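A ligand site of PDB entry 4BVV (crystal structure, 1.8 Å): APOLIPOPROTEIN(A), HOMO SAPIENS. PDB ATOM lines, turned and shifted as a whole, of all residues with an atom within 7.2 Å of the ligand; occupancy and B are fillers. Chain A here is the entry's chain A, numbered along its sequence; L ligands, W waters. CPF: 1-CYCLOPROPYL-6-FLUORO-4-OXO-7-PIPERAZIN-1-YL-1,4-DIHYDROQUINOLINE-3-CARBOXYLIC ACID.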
ATOM      1  N   TRP A  26      -2.985 -19.805 -19.615  1.00  0.00           N
ATOM      2  CA  TRP A  26      -1.547 -20.179 -19.503  1.00  0.00           C
ATOM      3  C   TRP A  26      -0.606 -19.045 -19.926  1.00  0.00           C
ATOM      4  O   TRP A  26       0.501 -18.903 -19.370  1.00  0.00           O
ATOM      5  CB  TRP A  26      -1.233 -21.466 -20.311  1.00  0.00           C
ATOM      6  CG  TRP A  26      -1.989 -22.703 -19.815  1.00  0.00           C
ATOM      7  CD1 TRP A  26      -3.158 -23.200 -20.319  1.00  0.00           C
ATOM      8  CD2 TRP A  26      -1.621 -23.558 -18.715  1.00  0.00           C
ATOM      9  NE1 TRP A  26      -3.538 -24.323 -19.597  1.00  0.00           N
ATOM     10  CE2 TRP A  26      -2.619 -24.563 -18.612  1.00  0.00           C
ATOM     11  CE3 TRP A  26      -0.535 -23.587 -17.813  1.00  0.00           C
ATOM     12  CZ2 TRP A  26      -2.577 -25.574 -17.643  1.00  0.00           C
ATOM     13  CZ3 TRP A  26      -0.502 -24.593 -16.843  1.00  0.00           C
ATOM     14  CH2 TRP A  26      -1.511 -25.574 -16.765  1.00  0.00           C
ATOM     15  N   ARG A  33       1.710 -14.621 -11.405  1.00  0.00           N
ATOM     16  CA  ARG A  33       2.951 -14.578 -12.183  1.00  0.00           C
ATOM     17  C   ARG A  33       3.586 -15.957 -12.177  1.00  0.00           C
ATOM     18  O   ARG A  33       3.574 -16.649 -11.156  1.00  0.00           O
ATOM     19  CB  ARG A  33       3.904 -13.536 -11.590  1.00  0.00           C
ATOM     20  CG  ARG A  33       3.500 -12.105 -11.884  1.00  0.00           C
ATOM     21  CD  ARG A  33       4.612 -11.084 -11.627  1.00  0.00           C
ATOM     22  NE  ARG A  33       5.876 -11.409 -12.291  1.00  0.00           N
ATOM     23  CZ  ARG A  33       6.953 -11.900 -11.681  1.00  0.00           C
ATOM     24  NH1 ARG A  33       6.923 -12.156 -10.368  1.00  0.00           N
ATOM     25  NH2 ARG A  33       8.064 -12.150 -12.366  1.00  0.00           N
ATOM     26  N   HIS A  34       4.115 -16.372 -13.326  1.00  0.00           N
ATOM     27  CA  HIS A  34       4.817 -17.642 -13.428  1.00  0.00           C
ATOM     28  C   HIS A  34       5.867 -17.657 -14.540  1.00  0.00           C
ATOM     29  O   HIS A  34       5.595 -17.298 -15.686  1.00  0.00           O
ATOM     30  CB  HIS A  34       3.815 -18.804 -13.594  1.00  0.00           C
ATOM     31  CG  HIS A  34       2.969 -18.707 -14.831  1.00  0.00           C
ATOM     32  ND1 HIS A  34       3.086 -19.579 -15.892  1.00  0.00           N
ATOM     33  CD2 HIS A  34       1.992 -17.837 -15.162  1.00  0.00           C
ATOM     34  CE1 HIS A  34       2.226 -19.253 -16.835  1.00  0.00           C
ATOM     35  NE2 HIS A  34       1.537 -18.195 -16.413  1.00  0.00           N
ATOM     36  N   SER A  35       7.086 -18.055 -14.169  1.00  0.00           N
ATOM     37  CA  SER A  35       8.197 -18.138 -15.103  1.00  0.00           C
ATOM     38  C   SER A  35       8.218 -19.490 -15.838  1.00  0.00           C
ATOM     39  O   SER A  35       8.869 -19.620 -16.874  1.00  0.00           O
ATOM     40  CB  SER A  35       9.524 -17.914 -14.382  1.00  0.00           C
ATOM     41  OG  SER A  35       9.813 -18.987 -13.499  1.00  0.00           O
ATOM     42  N   THR A  36       7.529 -20.479 -15.287  1.00  0.00           N
ATOM     43  CA  THR A  36       7.460 -21.817 -15.896  1.00  0.00           C
ATOM     44  C   THR A  36       6.070 -22.085 -16.470  1.00  0.00           C
ATOM     45  O   THR A  36       5.122 -21.376 -16.152  1.00  0.00           O
ATOM     46  CB  THR A  36       7.852 -22.919 -14.884  1.00  0.00           C
ATOM     47  OG1 THR A  36       6.865 -23.015 -13.855  1.00  0.00           O
ATOM     48  CG2 THR A  36       9.222 -22.629 -14.268  1.00  0.00           C
ATOM     49  N   PHE A  37       5.963 -23.117 -17.304  1.00  0.00           N
ATOM     50  CA  PHE A  37       4.701 -23.502 -17.946  1.00  0.00           C
ATOM     51  C   PHE A  37       4.077 -22.340 -18.749  1.00  0.00           C
ATOM     52  O   PHE A  37       2.898 -22.011 -18.569  1.00  0.00           O
ATOM     53  CB  PHE A  37       3.691 -24.105 -16.930  1.00  0.00           C
ATOM     54  CG  PHE A  37       4.253 -25.198 -16.044  1.00  0.00           C
ATOM     55  CD1 PHE A  37       4.757 -26.381 -16.600  1.00  0.00           C
ATOM     56  CD2 PHE A  37       4.248 -25.072 -14.660  1.00  0.00           C
ATOM     57  CE1 PHE A  37       5.253 -27.400 -15.785  1.00  0.00           C
ATOM     58  CE2 PHE A  37       4.753 -26.076 -13.834  1.00  0.00           C
ATOM     59  CZ  PHE A  37       5.257 -27.238 -14.401  1.00  0.00           C
ATOM     60  N   ASN A  54      -1.670 -31.252 -18.112  1.00  0.00           N
ATOM     61  CA  ASN A  54      -0.703 -31.887 -17.199  1.00  0.00           C
ATOM     62  C   ASN A  54       0.741 -31.886 -17.722  1.00  0.00           C
ATOM     63  O   ASN A  54       1.329 -32.954 -17.976  1.00  0.00           O
ATOM     64  CB  ASN A  54      -1.182 -33.300 -16.788  1.00  0.00           C
ATOM     65  CG  ASN A  54      -0.471 -33.864 -15.548  1.00  0.00           C
ATOM     66  OD1 ASN A  54       0.285 -33.177 -14.856  1.00  0.00           O
ATOM     67  ND2 ASN A  54      -0.721 -35.138 -15.245  1.00  0.00           N
ATOM     68  N   PRO A  55       1.344 -30.681 -17.887  1.00  0.00           N
ATOM     69  CA  PRO A  55       2.694 -30.574 -18.482  1.00  0.00           C
ATOM     70  C   PRO A  55       3.811 -31.299 -17.710  1.00  0.00           C
ATOM     71  O   PRO A  55       4.809 -31.682 -18.313  1.00  0.00           O
ATOM     72  CB  PRO A  55       2.965 -29.068 -18.504  1.00  0.00           C
ATOM     73  CG  PRO A  55       1.980 -28.452 -17.562  1.00  0.00           C
ATOM     74  CD  PRO A  55       0.783 -29.354 -17.560  1.00  0.00           C
ATOM     75  N   ASP A  56       3.640 -31.480 -16.392  1.00  0.00           N
ATOM     76  CA  ASP A  56       4.653 -32.170 -15.570  1.00  0.00           C
ATOM     77  C   ASP A  56       4.361 -33.653 -15.244  1.00  0.00           C
ATOM     78  O   ASP A  56       5.123 -34.277 -14.486  1.00  0.00           O
ATOM     79  CB  ASP A  56       4.984 -31.365 -14.297  1.00  0.00           C
ATOM     80  CG  ASP A  56       3.793 -31.157 -13.361  1.00  0.00           C
ATOM     81  OD1 ASP A  56       2.616 -31.355 -13.766  1.00  0.00           O
ATOM     82  OD2 ASP A  56       4.046 -30.788 -12.193  1.00  0.00           O
ATOM     83  N   GLY A  57       3.285 -34.205 -15.801  1.00  0.00           N
ATOM     84  CA  GLY A  57       2.928 -35.614 -15.546  1.00  0.00           C
ATOM     85  C   GLY A  57       2.653 -36.018 -14.100  1.00  0.00           C
ATOM     86  O   GLY A  57       3.044 -37.102 -13.657  1.00  0.00           O
ATOM     87  N   ASP A  58       1.989 -35.128 -13.353  1.00  0.00           N
ATOM     88  CA  ASP A  58       1.545 -35.357 -11.981  1.00  0.00           C
ATOM     89  C   ASP A  58       0.567 -36.551 -11.970  1.00  0.00           C
ATOM     90  O   ASP A  58      -0.398 -36.561 -12.744  1.00  0.00           O
ATOM     91  CB  ASP A  58       0.868 -34.070 -11.472  1.00  0.00           C
ATOM     92  CG  ASP A  58       0.614 -34.037  -9.971  1.00  0.00           C
ATOM     93  OD1 ASP A  58       0.152 -35.051  -9.374  1.00  0.00           O
ATOM     94  OD2 ASP A  58       0.838 -32.961  -9.365  1.00  0.00           O
ATOM     95  N   GLY A  61      -3.203 -35.967 -11.912  1.00  0.00           N
ATOM     96  CA  GLY A  61      -3.913 -35.636 -13.167  1.00  0.00           C
ATOM     97  C   GLY A  61      -3.877 -34.157 -13.588  1.00  0.00           C
ATOM     98  O   GLY A  61      -3.184 -33.350 -12.974  1.00  0.00           O
ATOM     99  N   TRP A  63      -4.482 -30.161 -14.346  1.00  0.00           N
ATOM    100  CA  TRP A  63      -4.586 -29.067 -13.379  1.00  0.00           C
ATOM    101  C   TRP A  63      -4.536 -27.709 -14.113  1.00  0.00           C
ATOM    102  O   TRP A  63      -4.345 -27.668 -15.329  1.00  0.00           O
ATOM    103  CB  TRP A  63      -3.474 -29.184 -12.319  1.00  0.00           C
ATOM    104  CG  TRP A  63      -2.064 -29.200 -12.886  1.00  0.00           C
ATOM    105  CD1 TRP A  63      -1.356 -30.309 -13.308  1.00  0.00           C
ATOM    106  CD2 TRP A  63      -1.209 -28.072 -13.121  1.00  0.00           C
ATOM    107  NE1 TRP A  63      -0.118 -29.932 -13.778  1.00  0.00           N
ATOM    108  CE2 TRP A  63       0.002 -28.569 -13.674  1.00  0.00           C
ATOM    109  CE3 TRP A  63      -1.336 -26.690 -12.907  1.00  0.00           C
ATOM    110  CZ2 TRP A  63       1.071 -27.733 -14.009  1.00  0.00           C
ATOM    111  CZ3 TRP A  63      -0.267 -25.854 -13.242  1.00  0.00           C
ATOM    112  CH2 TRP A  63       0.918 -26.379 -13.793  1.00  0.00           C
ATOM    113  N   CYS A  64      -4.749 -26.610 -13.386  1.00  0.00           N
ATOM    114  CA  CYS A  64      -4.581 -25.259 -13.939  1.00  0.00           C
ATOM    115  C   CYS A  64      -4.226 -24.224 -12.871  1.00  0.00           C
ATOM    116  O   CYS A  64      -4.463 -24.455 -11.694  1.00  0.00           O
ATOM    117  CB  CYS A  64      -5.853 -24.825 -14.694  1.00  0.00           C
ATOM    118  SG  CYS A  64      -7.303 -24.557 -13.639  1.00  0.00           S
ATOM    119  N   TYR A  65      -3.621 -23.105 -13.275  1.00  0.00           N
ATOM    120  CA  TYR A  65      -3.506 -21.935 -12.395  1.00  0.00           C
ATOM    121  C   TYR A  65      -4.925 -21.425 -12.128  1.00  0.00           C
ATOM    122  O   TYR A  65      -5.746 -21.409 -13.049  1.00  0.00           O
ATOM    123  CB  TYR A  65      -2.656 -20.827 -13.047  1.00  0.00           C
ATOM    124  CG  TYR A  65      -1.185 -21.161 -13.222  1.00  0.00           C
ATOM    125  CD1 TYR A  65      -0.265 -20.937 -12.184  1.00  0.00           C
ATOM    126  CD2 TYR A  65      -0.703 -21.681 -14.433  1.00  0.00           C
ATOM    127  CE1 TYR A  65       1.076 -21.239 -12.341  1.00  0.00           C
ATOM    128  CE2 TYR A  65       0.658 -21.987 -14.598  1.00  0.00           C
ATOM    129  CZ  TYR A  65       1.534 -21.761 -13.548  1.00  0.00           C
ATOM    130  OH  TYR A  65       2.881 -22.053 -13.685  1.00  0.00           O
ATOM    131  N   LEU A  72      -2.510 -20.535  -5.904  1.00  0.00           N
ATOM    132  CA  LEU A  72      -1.737 -20.696  -7.162  1.00  0.00           C
ATOM    133  C   LEU A  72      -2.340 -21.667  -8.200  1.00  0.00           C
ATOM    134  O   LEU A  72      -2.567 -21.286  -9.356  1.00  0.00           O
ATOM    135  CB  LEU A  72      -0.276 -21.062  -6.873  1.00  0.00           C
ATOM    136  CG  LEU A  72       0.667 -21.098  -8.097  1.00  0.00           C
ATOM    137  CD1 LEU A  72       0.919 -19.697  -8.634  1.00  0.00           C
ATOM    138  CD2 LEU A  72       1.981 -21.823  -7.817  1.00  0.00           C
ATOM    139  N   PHE A  73      -2.582 -22.913  -7.772  1.00  0.00           N
ATOM    140  CA  PHE A  73      -3.095 -23.957  -8.686  1.00  0.00           C
ATOM    141  C   PHE A  73      -4.080 -24.896  -7.974  1.00  0.00           C
ATOM    142  O   PHE A  73      -4.133 -24.956  -6.745  1.00  0.00           O
ATOM    143  CB  PHE A  73      -1.913 -24.758  -9.302  1.00  0.00           C
ATOM    144  CG  PHE A  73      -1.621 -26.067  -8.602  1.00  0.00           C
ATOM    145  CD1 PHE A  73      -0.864 -26.093  -7.431  1.00  0.00           C
ATOM    146  CD2 PHE A  73      -2.113 -27.271  -9.105  1.00  0.00           C
ATOM    147  CE1 PHE A  73      -0.615 -27.286  -6.782  1.00  0.00           C
ATOM    148  CE2 PHE A  73      -1.855 -28.469  -8.457  1.00  0.00           C
ATOM    149  CZ  PHE A  73      -1.100 -28.478  -7.289  1.00  0.00           C
ATOM    150  N   ASP A  74      -4.869 -25.638  -8.754  1.00  0.00           N
ATOM    151  CA  ASP A  74      -5.590 -26.792  -8.212  1.00  0.00           C
ATOM    152  C   ASP A  74      -5.798 -27.827  -9.300  1.00  0.00           C
ATOM    153  O   ASP A  74      -5.724 -27.497 -10.487  1.00  0.00           O
ATOM    154  CB  ASP A  74      -6.923 -26.381  -7.576  1.00  0.00           C
ATOM    155  CG  ASP A  74      -7.437 -27.398  -6.522  1.00  0.00           C
ATOM    156  OD1 ASP A  74      -6.814 -28.476  -6.323  1.00  0.00           O
ATOM    157  OD2 ASP A  74      -8.457 -27.104  -5.857  1.00  0.00           O
ATOM    158  N   TYR A  75      -6.030 -29.075  -8.895  1.00  0.00           N
ATOM    159  CA  TYR A  75      -6.399 -30.122  -9.842  1.00  0.00           C
ATOM    160  C   TYR A  75      -7.814 -29.929 -10.396  1.00  0.00           C
ATOM    161  O   TYR A  75      -8.675 -29.336  -9.742  1.00  0.00           O
ATOM    162  CB  TYR A  75      -6.255 -31.511  -9.216  1.00  0.00           C
ATOM    163  CG  TYR A  75      -4.847 -31.777  -8.742  1.00  0.00           C
ATOM    164  CD1 TYR A  75      -3.831 -32.124  -9.651  1.00  0.00           C
ATOM    165  CD2 TYR A  75      -4.517 -31.658  -7.402  1.00  0.00           C
ATOM    166  CE1 TYR A  75      -2.530 -32.353  -9.221  1.00  0.00           C
ATOM    167  CE2 TYR A  75      -3.218 -31.892  -6.963  1.00  0.00           C
ATOM    168  CZ  TYR A  75      -2.233 -32.232  -7.876  1.00  0.00           C
ATOM    169  OH  TYR A  75      -0.939 -32.454  -7.431  1.00  0.00           O
HETATM  170  O2  CPF L   1       8.508 -21.134 -10.797  1.00  0.00           O
HETATM  171  C3  CPF L   1       7.302 -21.276 -10.976  1.00  0.00           C
HETATM  172  O1  CPF L   1       6.624 -20.257 -11.520  1.00  0.00           O
HETATM  173  C2  CPF L   1       6.609 -22.535 -10.630  1.00  0.00           C
HETATM  174  C1  CPF L   1       7.314 -23.666 -10.214  1.00  0.00           C
HETATM  175  N1  CPF L   1       6.722 -24.839  -9.897  1.00  0.00           N
HETATM  176  C10 CPF L   1       5.348 -25.027  -9.995  1.00  0.00           C
HETATM  177  C9  CPF L   1       4.754 -26.265  -9.716  1.00  0.00           C
HETATM  178  C8  CPF L   1       3.368 -26.453  -9.805  1.00  0.00           C
HETATM  179  N2  CPF L   1       2.776 -27.708  -9.524  1.00  0.00           N
HETATM  180  C17 CPF L   1       3.765 -28.769  -9.181  1.00  0.00           C
HETATM  181  C16 CPF L   1       3.076 -30.121  -8.898  1.00  0.00           C
HETATM  182  N3  CPF L   1       2.221 -30.494 -10.041  1.00  0.00           N
HETATM  183  C15 CPF L   1       1.211 -29.455 -10.318  1.00  0.00           C
HETATM  184  C14 CPF L   1       1.961 -28.154 -10.673  1.00  0.00           C
HETATM  185  C7  CPF L   1       2.562 -25.344 -10.167  1.00  0.00           C
HETATM  186  F1  CPF L   1       1.217 -25.478 -10.249  1.00  0.00           F
HETATM  187  C6  CPF L   1       3.122 -24.126 -10.466  1.00  0.00           C
HETATM  188  C5  CPF L   1       4.508 -23.938 -10.377  1.00  0.00           C
HETATM  189  C4  CPF L   1       5.135 -22.635 -10.716  1.00  0.00           C
HETATM  190  O3  CPF L   1       4.470 -21.684 -11.118  1.00  0.00           O
HETATM  191  C11 CPF L   1       7.572 -25.956  -9.446  1.00  0.00           C
HETATM  192  C12 CPF L   1       8.779 -25.652  -8.534  1.00  0.00           C
HETATM  193  C13 CPF L   1       7.527 -26.296  -7.948  1.00  0.00           C
HETATM  194  O   HOH W   1       8.036 -17.383 -10.890  1.00  0.00           O
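An oxygen (O1) of the ligand sits at hydrogen-bond distance from the backbone NH (N) of Ser 35 (3.5 Å).
The side-chain carboxylate (OD2) of Asp 56 lies within salt-bridge range of a nitrogen (N3) of the ligand (2.8 Å).
An oxygen (O3) of the ligand sits at hydrogen-bond distance from the side-chain hydroxyl of Tyr 65, 3.0 Å away.
N3 of the ligand lies within salt-bridge range of OD2 of Asp 58 (2.9 Å).
OD1 of Asp 56 is in hydrogen-bond range of NE1 of Trp 63 (3.1 Å).
The side-chain hydroxyl (OH) of Tyr 65 is in hydrogen-bond range of a ring nitrogen (ND1) of His 34 (3.3 Å).
The side-chain amide oxygen of Asn 54 lies close to the side-chain carboxylate of Asp 56, 3.2 Å away.
NE2 of His 34 lies close to O of Trp 26 (3.2 Å).
NE1 of Trp 63 sits at hydrogen-bond distance from OD1 of Asn 54 (3.4 Å).
The side-chain hydroxyl of Tyr 65 is in hydrogen-bond range of the backbone carbonyl oxygen of Thr 36 (3.4 Å).
The side-chain carboxylate (OD2) of Asp 58 lies within hydrogen-bond range of the side-chain hydroxyl (OH) of Tyr 75 (2.7 Å).
The backbone carbonyl oxygen (O) of Asp 58 lies within hydrogen-bond range of the side-chain amide nitrogen (ND2) of Asn 54, at 2.9 Å.
CA of His 34 touches O1 of the ligand, 3.7 Å away.
Thr 36 touches the ligand (OG1 to C2, 3.3 Å).
CZ3 of Trp 63 touches F1 of the ligand (3.4 Å).
Leu 72 touches the ligand.
Phe 73 touches the ligand.
Water W1 lies within hydrogen-bond range of an oxygen (O1) of the ligand (3.3 Å) and the backbone NH of Ser 35 (3.5 Å).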
